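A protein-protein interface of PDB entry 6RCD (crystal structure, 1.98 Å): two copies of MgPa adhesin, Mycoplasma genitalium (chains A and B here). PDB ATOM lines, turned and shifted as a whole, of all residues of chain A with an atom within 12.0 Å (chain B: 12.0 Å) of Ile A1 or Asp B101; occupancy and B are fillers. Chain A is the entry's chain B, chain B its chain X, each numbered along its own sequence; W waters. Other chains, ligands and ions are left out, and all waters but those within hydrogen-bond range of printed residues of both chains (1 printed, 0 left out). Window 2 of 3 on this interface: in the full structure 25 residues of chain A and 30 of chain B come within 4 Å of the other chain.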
ATOM      1  N   ILE A   1     -17.734  36.547   4.900  1.00  0.00           N
ATOM      2  CA  ILE A   1     -17.580  36.364   3.450  1.00  0.00           C
ATOM      3  C   ILE A   1     -18.100  34.951   3.045  1.00  0.00           C
ATOM      4  O   ILE A   1     -19.251  34.844   2.616  1.00  0.00           O
ATOM      5  CB  ILE A   1     -16.126  36.720   2.970  1.00  0.00           C
ATOM      6  CG1 ILE A   1     -15.948  36.542   1.442  1.00  0.00           C
ATOM      7  CG2 ILE A   1     -15.030  35.984   3.763  1.00  0.00           C
ATOM      8  CD1 ILE A   1     -16.168  37.829   0.620  1.00  0.00           C
ATOM      9  N   SER A   2     -17.287  33.892   3.211  1.00  0.00           N
ATOM     10  CA  SER A   2     -17.680  32.502   2.956  1.00  0.00           C
ATOM     11  C   SER A   2     -17.517  31.695   4.230  1.00  0.00           C
ATOM     12  O   SER A   2     -16.495  31.795   4.901  1.00  0.00           O
ATOM     13  CB  SER A   2     -16.827  31.867   1.863  1.00  0.00           C
ATOM     14  OG  SER A   2     -16.928  32.602   0.660  1.00  0.00           O
ATOM     15  N   PHE A   3     -18.509  30.870   4.538  1.00  0.00           N
ATOM     16  CA  PHE A   3     -18.492  29.967   5.681  1.00  0.00           C
ATOM     17  C   PHE A   3     -17.704  28.711   5.263  1.00  0.00           C
ATOM     18  O   PHE A   3     -17.962  28.140   4.203  1.00  0.00           O
ATOM     19  CB  PHE A   3     -19.946  29.615   6.071  1.00  0.00           C
ATOM     20  CG  PHE A   3     -20.081  28.487   7.064  1.00  0.00           C
ATOM     21  CD1 PHE A   3     -19.682  28.650   8.382  1.00  0.00           C
ATOM     22  CD2 PHE A   3     -20.636  27.268   6.684  1.00  0.00           C
ATOM     23  CE1 PHE A   3     -19.830  27.612   9.302  1.00  0.00           C
ATOM     24  CE2 PHE A   3     -20.776  26.231   7.602  1.00  0.00           C
ATOM     25  CZ  PHE A   3     -20.365  26.408   8.905  1.00  0.00           C
ATOM     26  N   LYS A   4     -16.755  28.296   6.094  1.00  0.00           N
ATOM     27  CA  LYS A   4     -15.922  27.125   5.888  1.00  0.00           C
ATOM     28  C   LYS A   4     -16.130  26.245   7.092  1.00  0.00           C
ATOM     29  O   LYS A   4     -15.572  26.538   8.158  1.00  0.00           O
ATOM     30  CB  LYS A   4     -14.431  27.494   5.735  1.00  0.00           C
ATOM     31  CG  LYS A   4     -14.139  28.382   4.521  1.00  0.00           C
ATOM     32  CD  LYS A   4     -12.748  28.133   3.938  1.00  0.00           C
ATOM     33  CE  LYS A   4     -11.657  28.969   4.556  1.00  0.00           C
ATOM     34  NZ  LYS A   4     -11.575  30.299   3.907  1.00  0.00           N
ATOM     35  N   PRO A   5     -16.959  25.185   6.969  1.00  0.00           N
ATOM     36  CA  PRO A   5     -17.233  24.341   8.145  1.00  0.00           C
ATOM     37  C   PRO A   5     -16.030  23.583   8.674  1.00  0.00           C
ATOM     38  O   PRO A   5     -15.187  23.137   7.896  1.00  0.00           O
ATOM     39  CB  PRO A   5     -18.314  23.371   7.648  1.00  0.00           C
ATOM     40  CG  PRO A   5     -18.075  23.285   6.162  1.00  0.00           C
ATOM     41  CD  PRO A   5     -17.718  24.723   5.784  1.00  0.00           C
ATOM     42  N   VAL B  59      -1.451  28.040  10.242  1.00  0.00           N
ATOM     43  CA  VAL B  59      -2.026  29.256  10.831  1.00  0.00           C
ATOM     44  C   VAL B  59      -2.995  29.881   9.802  1.00  0.00           C
ATOM     45  O   VAL B  59      -4.095  30.300  10.162  1.00  0.00           O
ATOM     46  CB  VAL B  59      -0.909  30.252  11.279  1.00  0.00           C
ATOM     47  CG1 VAL B  59      -1.481  31.626  11.678  1.00  0.00           C
ATOM     48  CG2 VAL B  59      -0.076  29.651  12.419  1.00  0.00           C
ATOM     49  N   GLU B  60      -2.586  29.898   8.523  1.00  0.00           N
ATOM     50  CA  GLU B  60      -3.352  30.452   7.413  1.00  0.00           C
ATOM     51  C   GLU B  60      -4.682  29.741   7.208  1.00  0.00           C
ATOM     52  O   GLU B  60      -5.701  30.408   7.029  1.00  0.00           O
ATOM     53  CB  GLU B  60      -2.524  30.426   6.112  1.00  0.00           C
ATOM     54  CG  GLU B  60      -1.409  31.464   6.032  1.00  0.00           C
ATOM     55  CD  GLU B  60      -0.236  31.285   6.981  1.00  0.00           C
ATOM     56  OE1 GLU B  60       0.284  30.148   7.096  1.00  0.00           O
ATOM     57  OE2 GLU B  60       0.167  32.291   7.609  1.00  0.00           O
ATOM     58  N   ASN B  61      -4.695  28.397   7.253  1.00  0.00           N
ATOM     59  CA  ASN B  61      -5.921  27.622   7.037  1.00  0.00           C
ATOM     60  C   ASN B  61      -6.599  27.171   8.310  1.00  0.00           C
ATOM     61  O   ASN B  61      -7.692  26.607   8.244  1.00  0.00           O
ATOM     62  CB  ASN B  61      -5.653  26.428   6.110  1.00  0.00           C
ATOM     63  CG  ASN B  61      -5.096  26.836   4.763  1.00  0.00           C
ATOM     64  OD1 ASN B  61      -5.505  27.820   4.159  1.00  0.00           O
ATOM     65  ND2 ASN B  61      -4.144  26.097   4.273  1.00  0.00           N
ATOM     66  N   GLN B  62      -5.964  27.397   9.482  1.00  0.00           N
ATOM     67  CA  GLN B  62      -6.503  26.958  10.778  1.00  0.00           C
ATOM     68  C   GLN B  62      -6.771  25.436  10.770  1.00  0.00           C
ATOM     69  O   GLN B  62      -7.847  24.963  11.127  1.00  0.00           O
ATOM     70  CB  GLN B  62      -7.713  27.822  11.218  1.00  0.00           C
ATOM     71  CG  GLN B  62      -7.285  29.261  11.578  1.00  0.00           C
ATOM     72  CD  GLN B  62      -6.389  29.288  12.802  1.00  0.00           C
ATOM     73  OE1 GLN B  62      -6.750  28.781  13.861  1.00  0.00           O
ATOM     74  NE2 GLN B  62      -5.185  29.859  12.684  1.00  0.00           N
ATOM     75  N   GLN B  94      -9.729  20.789   9.871  1.00  0.00           N
ATOM     76  CA  GLN B  94      -9.988  22.149  10.360  1.00  0.00           C
ATOM     77  C   GLN B  94     -10.904  21.985  11.569  1.00  0.00           C
ATOM     78  O   GLN B  94     -12.072  21.671  11.385  1.00  0.00           O
ATOM     79  CB  GLN B  94     -10.647  22.969   9.249  1.00  0.00           C
ATOM     80  CG  GLN B  94     -10.918  24.426   9.614  1.00  0.00           C
ATOM     81  CD  GLN B  94     -11.863  25.019   8.612  1.00  0.00           C
ATOM     82  OE1 GLN B  94     -11.578  25.094   7.420  1.00  0.00           O
ATOM     83  NE2 GLN B  94     -13.022  25.451   9.068  1.00  0.00           N
ATOM     84  N   ASN B  97     -15.189  26.035  12.785  1.00  0.00           N
ATOM     85  CA  ASN B  97     -15.776  26.773  11.666  1.00  0.00           C
ATOM     86  C   ASN B  97     -14.970  28.051  11.447  1.00  0.00           C
ATOM     87  O   ASN B  97     -14.518  28.648  12.418  1.00  0.00           O
ATOM     88  CB  ASN B  97     -17.235  27.125  11.967  1.00  0.00           C
ATOM     89  CG  ASN B  97     -18.175  25.941  12.053  1.00  0.00           C
ATOM     90  OD1 ASN B  97     -17.959  24.877  11.452  1.00  0.00           O
ATOM     91  ND2 ASN B  97     -19.246  26.096  12.816  1.00  0.00           N
ATOM     92  N   GLN B  98     -14.720  28.415  10.175  1.00  0.00           N
ATOM     93  CA  GLN B  98     -13.968  29.623   9.817  1.00  0.00           C
ATOM     94  C   GLN B  98     -14.777  30.433   8.817  1.00  0.00           C
ATOM     95  O   GLN B  98     -15.595  29.868   8.087  1.00  0.00           O
ATOM     96  CB  GLN B  98     -12.576  29.287   9.217  1.00  0.00           C
ATOM     97  CG  GLN B  98     -11.636  28.443  10.119  1.00  0.00           C
ATOM     98  CD  GLN B  98     -11.232  29.122  11.419  1.00  0.00           C
ATOM     99  OE1 GLN B  98     -10.963  30.320  11.470  1.00  0.00           O
ATOM    100  NE2 GLN B  98     -11.147  28.371  12.500  1.00  0.00           N
ATOM    101  N   TRP B  99     -14.570  31.754   8.808  1.00  0.00           N
ATOM    102  CA  TRP B  99     -15.176  32.696   7.865  1.00  0.00           C
ATOM    103  C   TRP B  99     -14.010  33.436   7.234  1.00  0.00           C
ATOM    104  O   TRP B  99     -13.375  34.244   7.904  1.00  0.00           O
ATOM    105  CB  TRP B  99     -16.148  33.661   8.577  1.00  0.00           C
ATOM    106  CG  TRP B  99     -17.443  33.006   8.958  1.00  0.00           C
ATOM    107  CD1 TRP B  99     -18.599  32.991   8.230  1.00  0.00           C
ATOM    108  CD2 TRP B  99     -17.687  32.198  10.122  1.00  0.00           C
ATOM    109  NE1 TRP B  99     -19.563  32.266   8.893  1.00  0.00           N
ATOM    110  CE2 TRP B  99     -19.029  31.765  10.056  1.00  0.00           C
ATOM    111  CE3 TRP B  99     -16.911  31.829  11.237  1.00  0.00           C
ATOM    112  CZ2 TRP B  99     -19.606  30.958  11.052  1.00  0.00           C
ATOM    113  CZ3 TRP B  99     -17.479  31.036  12.222  1.00  0.00           C
ATOM    114  CH2 TRP B  99     -18.810  30.608  12.126  1.00  0.00           C
ATOM    115  N   ALA B 100     -13.639  33.072   6.006  1.00  0.00           N
ATOM    116  CA  ALA B 100     -12.503  33.684   5.298  1.00  0.00           C
ATOM    117  C   ALA B 100     -12.592  33.449   3.800  1.00  0.00           C
ATOM    118  O   ALA B 100     -13.249  32.500   3.367  1.00  0.00           O
ATOM    119  CB  ALA B 100     -11.175  33.140   5.831  1.00  0.00           C
ATOM    120  N   ASP B 101     -11.916  34.309   3.013  1.00  0.00           N
ATOM    121  CA  ASP B 101     -11.856  34.231   1.549  1.00  0.00           C
ATOM    122  C   ASP B 101     -10.964  33.070   1.104  1.00  0.00           C
ATOM    123  O   ASP B 101     -11.088  32.587  -0.021  1.00  0.00           O
ATOM    124  CB  ASP B 101     -11.341  35.553   0.955  1.00  0.00           C
ATOM    125  CG  ASP B 101     -12.413  36.611   0.806  1.00  0.00           C
ATOM    126  OD1 ASP B 101     -12.634  37.373   1.772  1.00  0.00           O
ATOM    127  OD2 ASP B 101     -13.032  36.680  -0.280  1.00  0.00           O
HETATM  128  O   HOH W   1     -14.111  32.142  -0.018  1.00  0.00           O
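Water W1 bridges the side-chain hydroxyl (OG) of Ser A2 (2.9 Å) and the backbone carbonyl oxygen (O) of Asp B101 (3.1 Å).
Of the 10 printed residues of chain B, 6 touch a printed residue of chain A.
Along chain B the printed residues that touch a printed residue of chain A span positions 94 to 101.
Of the 5 printed residues of chain A, 5 touch a printed residue of chain B.
Hydrophobic or aromatic side chains of chain A that line the printed part of chain B: Ile A1 and Phe A3.
Along chain A the printed residues that touch a printed residue of chain B span positions 1 to 5.
Among the printed residues, no Asp or Glu carboxylate lies within 4 Å of a Lys or Arg side-chain nitrogen of the other chain.
Among the printed residues, merely in contact across the chains: Ile A1 with Ala B100 (3.5 Å), Ile A1 with Asp B101 (3.4 Å), Ser A2 with Gln B98 (3.8 Å), Ser A2 with Trp B99 (3.4 Å), Phe A3 with Asn B97 (3.6 Å), Phe A3 with Gln B98 (3.7 Å), Phe A3 with Trp B99 (3.5 Å), Lys A4 with Asn B97 (3.5 Å), Lys A4 with Asp B101 (3.99 Å) and Pro A5 with Asn B97 (3.4 Å).
The backbone carbonyl oxygen (O) of Ser A2 is in hydrogen-bond range of the backbone NH (N) of Ala B100, 3.3 Å away.
The backbone carbonyl oxygen (O) of Lys A4 is in hydrogen-bond range of the side-chain amide nitrogen (NE2) of Gln B94.
The backbone carbonyl oxygen (O) of Gln B98 is in hydrogen-bond range of the backbone NH (N) of Lys A4, at 2.8 Å.
The side-chain amino group of Lys A4 is in hydrogen-bond range of the backbone carbonyl oxygen of Ala B100 (2.8 Å).
The backbone carbonyl oxygen (O) of Pro A5 is in hydrogen-bond range of the side-chain amide nitrogen (NE2) of Gln B94 (3.4 Å).
No position is printed for both chains.
Of the 15 pairs that touch across the chains among the printed residues, none has its exchanged pair printed and touching as well.
Of chain B, only Ala B100 (3.5 Å) and Asp B101 (3.4 Å) come within 4 Å of Ile A1.
Printed residues of chain B within 4 Å of Ser A2: Gln B98 (3.8 Å), Trp B99 (3.4 Å) and Ala B100 (3.3 Å).
Printed residues of chain B within 4 Å of Phe A3: Asn B97 (3.6 Å), Gln B98 (3.7 Å) and Trp B99 (3.5 Å).
Of the printed residues of chain B, Lys A4 touches Gln B94 (2.9 Å), Asn B97 (3.5 Å), Gln B98 (2.8 Å), Ala B100 (2.8 Å) and Asp B101 (3.99 Å).
Of the printed residues of chain B, Pro A5 touches Gln B94 and Asn B97.
Val B59 touches none of the printed residues of chain A.
Of the printed residues of chain A, Gln B94 touches Lys A4 and Pro A5.
Of the printed residues of chain A, Asn B97 touches Phe A3, Lys A4 and Pro A5.
Of chain A, only Ile A1 (3.5 Å), Ser A2 (3.3 Å) and Lys A4 (2.8 Å) come within 4 Å of Ala B100.
Of the printed residues of chain A, Asp B101 touches Ile A1 and Lys A4.
The nearest printed residue of chain A that does not touch Asp B101 is Ser A2 (5.4 Å).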
